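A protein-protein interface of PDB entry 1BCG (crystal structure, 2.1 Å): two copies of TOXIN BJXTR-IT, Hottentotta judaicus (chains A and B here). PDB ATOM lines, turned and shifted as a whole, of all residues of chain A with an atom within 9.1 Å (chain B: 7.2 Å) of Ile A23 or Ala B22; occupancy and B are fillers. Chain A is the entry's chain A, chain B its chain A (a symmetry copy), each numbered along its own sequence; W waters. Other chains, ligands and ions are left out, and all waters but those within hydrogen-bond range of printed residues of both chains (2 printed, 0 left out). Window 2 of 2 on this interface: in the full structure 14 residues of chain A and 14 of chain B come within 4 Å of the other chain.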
ATOM      1  N   CYS A  17      19.491  -2.969  35.087  1.00  0.00           N
ATOM      2  CA  CYS A  17      18.997  -4.229  34.547  1.00  0.00           C
ATOM      3  C   CYS A  17      20.102  -5.273  34.654  1.00  0.00           C
ATOM      4  O   CYS A  17      21.229  -5.054  34.217  1.00  0.00           O
ATOM      5  CB  CYS A  17      18.521  -4.045  33.093  1.00  0.00           C
ATOM      6  SG  CYS A  17      19.644  -3.143  31.970  1.00  0.00           S
ATOM      7  N   SER A  18      19.781  -6.400  35.278  1.00  0.00           N
ATOM      8  CA  SER A  18      20.759  -7.463  35.453  1.00  0.00           C
ATOM      9  C   SER A  18      20.075  -8.818  35.490  1.00  0.00           C
ATOM     10  O   SER A  18      18.846  -8.905  35.472  1.00  0.00           O
ATOM     11  CB  SER A  18      21.540  -7.248  36.750  1.00  0.00           C
ATOM     12  OG  SER A  18      20.664  -7.247  37.865  1.00  0.00           O
ATOM     13  N   GLY A  19      20.883  -9.874  35.539  1.00  0.00           N
ATOM     14  CA  GLY A  19      20.339 -11.212  35.572  1.00  0.00           C
ATOM     15  C   GLY A  19      19.564 -11.507  34.308  1.00  0.00           C
ATOM     16  O   GLY A  19      20.029 -11.221  33.203  1.00  0.00           O
ATOM     17  N   VAL A  20      18.372 -12.072  34.470  1.00  0.00           N
ATOM     18  CA  VAL A  20      17.538 -12.414  33.328  1.00  0.00           C
ATOM     19  C   VAL A  20      17.101 -11.172  32.556  1.00  0.00           C
ATOM     20  O   VAL A  20      16.811 -11.252  31.359  1.00  0.00           O
ATOM     21  CB  VAL A  20      16.280 -13.205  33.771  1.00  0.00           C
ATOM     22  CG1 VAL A  20      15.455 -12.379  34.744  1.00  0.00           C
ATOM     23  CG2 VAL A  20      15.450 -13.586  32.549  1.00  0.00           C
ATOM     24  N   ASN A  21      17.055 -10.024  33.225  1.00  0.00           N
ATOM     25  CA  ASN A  21      16.652  -8.808  32.532  1.00  0.00           C
ATOM     26  C   ASN A  21      17.795  -8.133  31.782  1.00  0.00           C
ATOM     27  O   ASN A  21      17.609  -7.095  31.144  1.00  0.00           O
ATOM     28  CB  ASN A  21      15.970  -7.833  33.492  1.00  0.00           C
ATOM     29  CG  ASN A  21      14.631  -8.361  33.985  1.00  0.00           C
ATOM     30  OD1 ASN A  21      13.899  -9.012  33.234  1.00  0.00           O
ATOM     31  ND2 ASN A  21      14.293  -8.068  35.229  1.00  0.00           N
ATOM     32  N   ALA A  22      18.975  -8.743  31.853  1.00  0.00           N
ATOM     33  CA  ALA A  22      20.144  -8.239  31.148  1.00  0.00           C
ATOM     34  C   ALA A  22      20.329  -9.099  29.904  1.00  0.00           C
ATOM     35  O   ALA A  22      20.883  -8.647  28.907  1.00  0.00           O
ATOM     36  CB  ALA A  22      21.386  -8.326  32.028  1.00  0.00           C
ATOM     37  N   ILE A  23      19.856 -10.340  29.965  1.00  0.00           N
ATOM     38  CA  ILE A  23      19.988 -11.252  28.833  1.00  0.00           C
ATOM     39  C   ILE A  23      18.836 -11.121  27.837  1.00  0.00           C
ATOM     40  O   ILE A  23      19.031 -11.267  26.635  1.00  0.00           O
ATOM     41  CB  ILE A  23      20.095 -12.728  29.302  1.00  0.00           C
ATOM     42  CG1 ILE A  23      20.304 -13.640  28.090  1.00  0.00           C
ATOM     43  CG2 ILE A  23      18.836 -13.136  30.054  1.00  0.00           C
ATOM     44  CD1 ILE A  23      20.480 -15.108  28.436  1.00  0.00           C
ATOM     45  N   ALA A  24      17.638 -10.841  28.338  1.00  0.00           N
ATOM     46  CA  ALA A  24      16.465 -10.679  27.478  1.00  0.00           C
ATOM     47  C   ALA A  24      16.078  -9.199  27.465  1.00  0.00           C
ATOM     48  O   ALA A  24      16.090  -8.545  28.505  1.00  0.00           O
ATOM     49  CB  ALA A  24      15.314 -11.525  28.001  1.00  0.00           C
ATOM     50  N   PRO A  25      15.713  -8.658  26.286  1.00  0.00           N
ATOM     51  CA  PRO A  25      15.320  -7.255  26.089  1.00  0.00           C
ATOM     52  C   PRO A  25      13.972  -6.851  26.683  1.00  0.00           C
ATOM     53  O   PRO A  25      13.717  -5.673  26.910  1.00  0.00           O
ATOM     54  CB  PRO A  25      15.287  -7.120  24.561  1.00  0.00           C
ATOM     55  CG  PRO A  25      16.113  -8.304  24.069  1.00  0.00           C
ATOM     56  CD  PRO A  25      15.630  -9.371  25.003  1.00  0.00           C
ATOM     57  N   HIS A  26      13.112  -7.834  26.924  1.00  0.00           N
ATOM     58  CA  HIS A  26      11.758  -7.583  27.414  1.00  0.00           C
ATOM     59  C   HIS A  26      11.570  -6.586  28.552  1.00  0.00           C
ATOM     60  O   HIS A  26      10.726  -5.691  28.460  1.00  0.00           O
ATOM     61  CB  HIS A  26      11.102  -8.915  27.760  1.00  0.00           C
ATOM     62  CG  HIS A  26      11.081  -9.877  26.616  1.00  0.00           C
ATOM     63  ND1 HIS A  26      12.231 -10.413  26.074  1.00  0.00           N
ATOM     64  CD2 HIS A  26      10.057 -10.355  25.870  1.00  0.00           C
ATOM     65  CE1 HIS A  26      11.915 -11.181  25.048  1.00  0.00           C
ATOM     66  NE2 HIS A  26      10.602 -11.164  24.902  1.00  0.00           N
ATOM     67  N   TYR A  27      12.335  -6.728  29.627  1.00  0.00           N
ATOM     68  CA  TYR A  27      12.204  -5.806  30.744  1.00  0.00           C
ATOM     69  C   TYR A  27      12.435  -4.365  30.293  1.00  0.00           C
ATOM     70  O   TYR A  27      11.555  -3.509  30.423  1.00  0.00           O
ATOM     71  CB  TYR A  27      13.201  -6.158  31.846  1.00  0.00           C
ATOM     72  CG  TYR A  27      13.217  -5.157  32.972  1.00  0.00           C
ATOM     73  CD1 TYR A  27      12.095  -4.964  33.779  1.00  0.00           C
ATOM     74  CD2 TYR A  27      14.346  -4.375  33.213  1.00  0.00           C
ATOM     75  CE1 TYR A  27      12.099  -4.012  34.798  1.00  0.00           C
ATOM     76  CE2 TYR A  27      14.360  -3.423  34.227  1.00  0.00           C
ATOM     77  CZ  TYR A  27      13.236  -3.247  35.013  1.00  0.00           C
ATOM     78  OH  TYR A  27      13.249  -2.301  36.012  1.00  0.00           O
ATOM     79  N   CYS A  28      13.623  -4.100  29.762  1.00  0.00           N
ATOM     80  CA  CYS A  28      13.948  -2.757  29.304  1.00  0.00           C
ATOM     81  C   CYS A  28      13.060  -2.263  28.164  1.00  0.00           C
ATOM     82  O   CYS A  28      12.791  -1.066  28.063  1.00  0.00           O
ATOM     83  CB  CYS A  28      15.419  -2.680  28.890  1.00  0.00           C
ATOM     84  SG  CYS A  28      16.564  -2.735  30.307  1.00  0.00           S
ATOM     85  N   TYR A  42      16.526  -2.086  25.276  1.00  0.00           N
ATOM     86  CA  TYR A  42      17.131  -3.320  25.758  1.00  0.00           C
ATOM     87  C   TYR A  42      18.134  -2.951  26.844  1.00  0.00           C
ATOM     88  O   TYR A  42      18.324  -1.767  27.136  1.00  0.00           O
ATOM     89  CB  TYR A  42      17.804  -4.082  24.605  1.00  0.00           C
ATOM     90  CG  TYR A  42      19.122  -3.516  24.096  1.00  0.00           C
ATOM     91  CD1 TYR A  42      19.153  -2.431  23.224  1.00  0.00           C
ATOM     92  CD2 TYR A  42      20.336  -4.105  24.455  1.00  0.00           C
ATOM     93  CE1 TYR A  42      20.369  -1.947  22.715  1.00  0.00           C
ATOM     94  CE2 TYR A  42      21.549  -3.635  23.955  1.00  0.00           C
ATOM     95  CZ  TYR A  42      21.560  -2.561  23.085  1.00  0.00           C
ATOM     96  OH  TYR A  42      22.759  -2.120  22.574  1.00  0.00           O
ATOM     97  N   CYS A  43      18.755  -3.953  27.454  1.00  0.00           N
ATOM     98  CA  CYS A  43      19.723  -3.711  28.513  1.00  0.00           C
ATOM     99  C   CYS A  43      21.115  -3.551  27.918  1.00  0.00           C
ATOM    100  O   CYS A  43      21.686  -4.516  27.398  1.00  0.00           O
ATOM    101  CB  CYS A  43      19.734  -4.879  29.502  1.00  0.00           C
ATOM    102  SG  CYS A  43      20.705  -4.584  31.019  1.00  0.00           S
ATOM    103  N   CYS A  44      21.652  -2.335  27.972  1.00  0.00           N
ATOM    104  CA  CYS A  44      22.991  -2.090  27.453  1.00  0.00           C
ATOM    105  C   CYS A  44      23.911  -1.756  28.624  1.00  0.00           C
ATOM    106  O   CYS A  44      23.808  -0.695  29.231  1.00  0.00           O
ATOM    107  CB  CYS A  44      23.028  -0.920  26.465  1.00  0.00           C
ATOM    108  SG  CYS A  44      24.633  -0.844  25.600  1.00  0.00           S
ATOM    109  N   GLY A  46      24.218  -2.982  31.845  1.00  0.00           N
ATOM    110  CA  GLY A  46      23.648  -2.751  33.159  1.00  0.00           C
ATOM    111  C   GLY A  46      22.546  -1.723  33.316  1.00  0.00           C
ATOM    112  O   GLY A  46      22.088  -1.503  34.436  1.00  0.00           O
ATOM    113  N   TYR A  69      28.440   1.619  20.949  1.00  0.00           N
ATOM    114  CA  TYR A  69      28.224   0.235  21.343  1.00  0.00           C
ATOM    115  C   TYR A  69      26.736  -0.051  21.577  1.00  0.00           C
ATOM    116  O   TYR A  69      26.224  -1.082  21.158  1.00  0.00           O
ATOM    117  CB  TYR A  69      28.985  -0.060  22.631  1.00  0.00           C
ATOM    118  CG  TYR A  69      28.686  -1.414  23.232  1.00  0.00           C
ATOM    119  CD1 TYR A  69      29.209  -2.582  22.679  1.00  0.00           C
ATOM    120  CD2 TYR A  69      27.877  -1.527  24.366  1.00  0.00           C
ATOM    121  CE1 TYR A  69      28.939  -3.829  23.246  1.00  0.00           C
ATOM    122  CE2 TYR A  69      27.602  -2.765  24.937  1.00  0.00           C
ATOM    123  CZ  TYR A  69      28.138  -3.909  24.374  1.00  0.00           C
ATOM    124  OH  TYR A  69      27.882  -5.132  24.951  1.00  0.00           O
ATOM    125  N   CYS B  17      24.246 -19.103  19.966  1.00  0.00           N
ATOM    126  CA  CYS B  17      24.798 -17.911  20.598  1.00  0.00           C
ATOM    127  C   CYS B  17      24.724 -18.082  22.110  1.00  0.00           C
ATOM    128  O   CYS B  17      23.672 -18.390  22.665  1.00  0.00           O
ATOM    129  CB  CYS B  17      24.048 -16.651  20.125  1.00  0.00           C
ATOM    130  SG  CYS B  17      22.223 -16.727  20.145  1.00  0.00           S
ATOM    131  N   SER B  18      25.864 -17.917  22.772  1.00  0.00           N
ATOM    132  CA  SER B  18      25.918 -18.070  24.218  1.00  0.00           C
ATOM    133  C   SER B  18      27.001 -17.186  24.808  1.00  0.00           C
ATOM    134  O   SER B  18      27.755 -16.538  24.078  1.00  0.00           O
ATOM    135  CB  SER B  18      26.194 -19.530  24.581  1.00  0.00           C
ATOM    136  OG  SER B  18      27.429 -19.955  24.032  1.00  0.00           O
ATOM    137  N   GLY B  19      27.070 -17.162  26.136  1.00  0.00           N
ATOM    138  CA  GLY B  19      28.061 -16.350  26.805  1.00  0.00           C
ATOM    139  C   GLY B  19      27.841 -14.885  26.507  1.00  0.00           C
ATOM    140  O   GLY B  19      26.713 -14.390  26.572  1.00  0.00           O
ATOM    141  N   VAL B  20      28.921 -14.187  26.169  1.00  0.00           N
ATOM    142  CA  VAL B  20      28.838 -12.765  25.870  1.00  0.00           C
ATOM    143  C   VAL B  20      27.992 -12.497  24.628  1.00  0.00           C
ATOM    144  O   VAL B  20      27.427 -11.410  24.481  1.00  0.00           O
ATOM    145  CB  VAL B  20      30.248 -12.154  25.667  1.00  0.00           C
ATOM    146  CG1 VAL B  20      30.962 -12.849  24.519  1.00  0.00           C
ATOM    147  CG2 VAL B  20      30.129 -10.656  25.399  1.00  0.00           C
ATOM    148  N   ASN B  21      27.896 -13.477  23.735  1.00  0.00           N
ATOM    149  CA  ASN B  21      27.093 -13.275  22.536  1.00  0.00           C
ATOM    150  C   ASN B  21      25.609 -13.547  22.748  1.00  0.00           C
ATOM    151  O   ASN B  21      24.802 -13.416  21.827  1.00  0.00           O
ATOM    152  CB  ASN B  21      27.643 -14.094  21.367  1.00  0.00           C
ATOM    153  CG  ASN B  21      29.006 -13.593  20.911  1.00  0.00           C
ATOM    154  OD1 ASN B  21      29.266 -12.387  20.921  1.00  0.00           O
ATOM    155  ND2 ASN B  21      29.868 -14.503  20.490  1.00  0.00           N
ATOM    156  N   ALA B  22      25.257 -13.913  23.979  1.00  0.00           N
ATOM    157  CA  ALA B  22      23.869 -14.158  24.339  1.00  0.00           C
ATOM    158  C   ALA B  22      23.372 -12.932  25.093  1.00  0.00           C
ATOM    159  O   ALA B  22      22.182 -12.634  25.091  1.00  0.00           O
ATOM    160  CB  ALA B  22      23.751 -15.395  25.224  1.00  0.00           C
ATOM    161  N   ILE B  23      24.292 -12.216  25.734  1.00  0.00           N
ATOM    162  CA  ILE B  23      23.924 -11.027  26.496  1.00  0.00           C
ATOM    163  C   ILE B  23      23.893  -9.765  25.634  1.00  0.00           C
ATOM    164  O   ILE B  23      23.071  -8.881  25.852  1.00  0.00           O
ATOM    165  CB  ILE B  23      24.881 -10.803  27.698  1.00  0.00           C
ATOM    166  CG1 ILE B  23      24.416  -9.590  28.507  1.00  0.00           C
ATOM    167  CG2 ILE B  23      26.306 -10.590  27.207  1.00  0.00           C
ATOM    168  CD1 ILE B  23      25.249  -9.309  29.746  1.00  0.00           C
ATOM    169  N   ALA B  24      24.786  -9.685  24.654  1.00  0.00           N
ATOM    170  CA  ALA B  24      24.840  -8.530  23.757  1.00  0.00           C
ATOM    171  C   ALA B  24      24.342  -8.967  22.378  1.00  0.00           C
ATOM    172  O   ALA B  24      24.690 -10.046  21.905  1.00  0.00           O
ATOM    173  CB  ALA B  24      26.266  -8.008  23.664  1.00  0.00           C
ATOM    174  N   PRO B  25      23.531  -8.124  21.710  1.00  0.00           N
ATOM    175  CA  PRO B  25      22.954  -8.384  20.383  1.00  0.00           C
ATOM    176  C   PRO B  25      23.935  -8.356  19.213  1.00  0.00           C
ATOM    177  O   PRO B  25      23.659  -8.911  18.153  1.00  0.00           O
ATOM    178  CB  PRO B  25      21.918  -7.261  20.233  1.00  0.00           C
ATOM    179  CG  PRO B  25      21.689  -6.780  21.661  1.00  0.00           C
ATOM    180  CD  PRO B  25      23.095  -6.799  22.178  1.00  0.00           C
ATOM    181  N   TYR B  27      26.743  -9.858  18.108  1.00  0.00           N
ATOM    182  CA  TYR B  27      27.095 -11.041  17.339  1.00  0.00           C
ATOM    183  C   TYR B  27      25.968 -11.427  16.383  1.00  0.00           C
ATOM    184  O   TYR B  27      26.154 -11.466  15.164  1.00  0.00           O
ATOM    185  CB  TYR B  27      27.393 -12.214  18.271  1.00  0.00           C
ATOM    186  CG  TYR B  27      27.626 -13.509  17.537  1.00  0.00           C
ATOM    187  CD1 TYR B  27      28.714 -13.662  16.677  1.00  0.00           C
ATOM    188  CD2 TYR B  27      26.740 -14.576  17.676  1.00  0.00           C
ATOM    189  CE1 TYR B  27      28.911 -14.849  15.972  1.00  0.00           C
ATOM    190  CE2 TYR B  27      26.925 -15.763  16.977  1.00  0.00           C
ATOM    191  CZ  TYR B  27      28.010 -15.892  16.128  1.00  0.00           C
ATOM    192  OH  TYR B  27      28.190 -17.066  15.432  1.00  0.00           O
ATOM    193  N   CYS B  28      24.797 -11.713  16.941  1.00  0.00           N
ATOM    194  CA  CYS B  28      23.658 -12.097  16.120  1.00  0.00           C
ATOM    195  C   CYS B  28      23.203 -11.010  15.150  1.00  0.00           C
ATOM    196  O   CYS B  28      22.715 -11.315  14.062  1.00  0.00           O
ATOM    197  CB  CYS B  28      22.488 -12.529  17.007  1.00  0.00           C
ATOM    198  SG  CYS B  28      22.759 -14.141  17.813  1.00  0.00           S
ATOM    199  N   TYR B  42      19.210 -10.566  17.211  1.00  0.00           N
ATOM    200  CA  TYR B  42      19.765 -10.698  18.550  1.00  0.00           C
ATOM    201  C   TYR B  42      19.699 -12.170  18.936  1.00  0.00           C
ATOM    202  O   TYR B  42      19.202 -12.993  18.162  1.00  0.00           O
ATOM    203  CB  TYR B  42      18.992  -9.819  19.547  1.00  0.00           C
ATOM    204  CG  TYR B  42      17.614 -10.313  19.961  1.00  0.00           C
ATOM    205  CD1 TYR B  42      16.505 -10.129  19.140  1.00  0.00           C
ATOM    206  CD2 TYR B  42      17.419 -10.923  21.201  1.00  0.00           C
ATOM    207  CE1 TYR B  42      15.225 -10.538  19.549  1.00  0.00           C
ATOM    208  CE2 TYR B  42      16.153 -11.333  21.620  1.00  0.00           C
ATOM    209  CZ  TYR B  42      15.063 -11.135  20.794  1.00  0.00           C
ATOM    210  OH  TYR B  42      13.813 -11.516  21.226  1.00  0.00           O
ATOM    211  N   CYS B  43      20.215 -12.507  20.113  1.00  0.00           N
ATOM    212  CA  CYS B  43      20.214 -13.887  20.572  1.00  0.00           C
ATOM    213  C   CYS B  43      18.933 -14.178  21.341  1.00  0.00           C
ATOM    214  O   CYS B  43      18.729 -13.645  22.438  1.00  0.00           O
ATOM    215  CB  CYS B  43      21.414 -14.145  21.486  1.00  0.00           C
ATOM    216  SG  CYS B  43      21.682 -15.899  21.915  1.00  0.00           S
ATOM    217  N   CYS B  44      18.063 -15.001  20.763  1.00  0.00           N
ATOM    218  CA  CYS B  44      16.820 -15.360  21.435  1.00  0.00           C
ATOM    219  C   CYS B  44      16.876 -16.842  21.795  1.00  0.00           C
ATOM    220  O   CYS B  44      16.814 -17.710  20.930  1.00  0.00           O
ATOM    221  CB  CYS B  44      15.591 -15.127  20.551  1.00  0.00           C
ATOM    222  SG  CYS B  44      14.051 -15.279  21.517  1.00  0.00           S
ATOM    223  N   TRP B  45      17.017 -17.111  23.082  1.00  0.00           N
ATOM    224  CA  TRP B  45      17.072 -18.468  23.601  1.00  0.00           C
ATOM    225  C   TRP B  45      18.129 -19.376  22.986  1.00  0.00           C
ATOM    226  O   TRP B  45      17.823 -20.469  22.521  1.00  0.00           O
ATOM    227  CB  TRP B  45      15.702 -19.135  23.475  1.00  0.00           C
ATOM    228  CG  TRP B  45      15.485 -20.099  24.581  1.00  0.00           C
ATOM    229  CD1 TRP B  45      15.416 -21.463  24.496  1.00  0.00           C
ATOM    230  CD2 TRP B  45      15.392 -19.776  25.968  1.00  0.00           C
ATOM    231  NE1 TRP B  45      15.285 -22.004  25.753  1.00  0.00           N
ATOM    232  CE2 TRP B  45      15.268 -20.990  26.674  1.00  0.00           C
ATOM    233  CE3 TRP B  45      15.400 -18.571  26.685  1.00  0.00           C
ATOM    234  CZ2 TRP B  45      15.155 -21.037  28.066  1.00  0.00           C
ATOM    235  CZ3 TRP B  45      15.288 -18.617  28.070  1.00  0.00           C
ATOM    236  CH2 TRP B  45      15.167 -19.845  28.742  1.00  0.00           C
ATOM    237  N   GLY B  46      19.374 -18.920  22.982  1.00  0.00           N
ATOM    238  CA  GLY B  46      20.448 -19.744  22.459  1.00  0.00           C
ATOM    239  C   GLY B  46      20.699 -19.770  20.964  1.00  0.00           C
ATOM    240  O   GLY B  46      21.586 -20.495  20.519  1.00  0.00           O
ATOM    241  N   TYR B  69       7.607 -14.637  22.027  1.00  0.00           N
ATOM    242  CA  TYR B  69       8.661 -14.239  22.948  1.00  0.00           C
ATOM    243  C   TYR B  69       9.826 -13.573  22.207  1.00  0.00           C
ATOM    244  O   TYR B  69      10.356 -12.564  22.654  1.00  0.00           O
ATOM    245  CB  TYR B  69       9.190 -15.464  23.687  1.00  0.00           C
ATOM    246  CG  TYR B  69      10.412 -15.196  24.535  1.00  0.00           C
ATOM    247  CD1 TYR B  69      10.313 -14.528  25.754  1.00  0.00           C
ATOM    248  CD2 TYR B  69      11.677 -15.620  24.116  1.00  0.00           C
ATOM    249  CE1 TYR B  69      11.444 -14.295  26.540  1.00  0.00           C
ATOM    250  CE2 TYR B  69      12.808 -15.391  24.892  1.00  0.00           C
ATOM    251  CZ  TYR B  69      12.684 -14.731  26.101  1.00  0.00           C
ATOM    252  OH  TYR B  69      13.801 -14.523  26.876  1.00  0.00           O
HETATM  253  O   HOH W   1      17.719 -12.699  24.728  1.00  0.00           O
HETATM  254  O   HOH W   2      23.303  -6.177  26.062  1.00  0.00           O
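O of Tyr B69 lies within hydrogen-bond range of NE2 of His A26 (2.7 Å).
The side-chain hydroxyl (OH) of Tyr A42 is in hydrogen-bond range of the side-chain sulfur (SG) of Cys A44, at 3.8 Å. SG of Cys A43 is disulfide-bonded to SG of Cys A17. SG of Cys B43 forms a disulfide with SG of Cys B17, at 2.0 Å. OH of Tyr B42 is in hydrogen-bond range of SG of Cys B44 (3.8 Å).
O of Ala A22 touches CG1 of Ile B23, 3.7 Å away. CG1 of Ile A23 touches O of Ala B22, 3.7 Å away. Tyr B69 touches Ala A24 (OH to CB, 3.5 Å). Tyr B42 touches Pro A25 (CE2 to CG, 3.9 Å). CG of Pro B25 touches CE2 of Tyr A42, at 3.9 Å. OH of Tyr A69 touches CB of Ala B24, at 3.5 Å.
Ile A23 touches just one residue of chain B: Ala B22 (3.7 Å). Of the printed residues of chain B, His A26 touches Tyr B69 (2.7 Å). Printed residues of chain B within 4 Å of Tyr A42: Pro B25 (3.9 Å). Printed residues of chain B within 4 Å of Tyr A69: Ala B24 (3.5 Å). Cys B17 touches none of the printed residues of chain A. Gly B19 touches none of the printed residues of chain A. Printed residues of chain A within 4 Å of Pro B25: Tyr A42 (3.9 Å). Cys B44 touches none of the printed residues of chain A. The nearest residue of chain B that does not touch Ile A23 is Ile B23 (4.6 Å). The nearest printed residue of chain B that does not touch Tyr A69 is Pro B25 (5.8 Å).
Of the 17 printed residues of chain A, 7 touch a printed residue of chain B. Hydrophobic or aromatic side chains of chain A that line the printed part of chain B: Ile A23, Ala A24, Pro A25, His A26, Tyr A42 and Tyr A69. Of the 17 printed residues of chain B, 6 touch a printed residue of chain A. Among the printed residues, no Asp or Glu carboxylate lies within 4 Å of a Lys or Arg side-chain nitrogen of the other chain.
Ala A22 touches Ile B23, and with the chains exchanged Ile A23 touches Ala B22. Ala A24 touches Tyr B69, and with the chains exchanged Tyr A69 touches Ala B24. Pro A25 touches Tyr B42, and with the chains exchanged Tyr A42 touches Pro B25. Positions printed for both chains: 17, 18, 19, 20, 21, 22, 23, 24, 25, 27, 28, 42, 43, 44, 46 and 69.
Water W2 lies within hydrogen-bond range of O of Cys A43 (2.7 Å) and O of Ile B23 (2.7 Å). Water W1 lies within hydrogen-bond range of the backbone carbonyl oxygen of Cys B43 (2.7 Å) and the backbone carbonyl oxygen of Ile A23 (2.7 Å).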
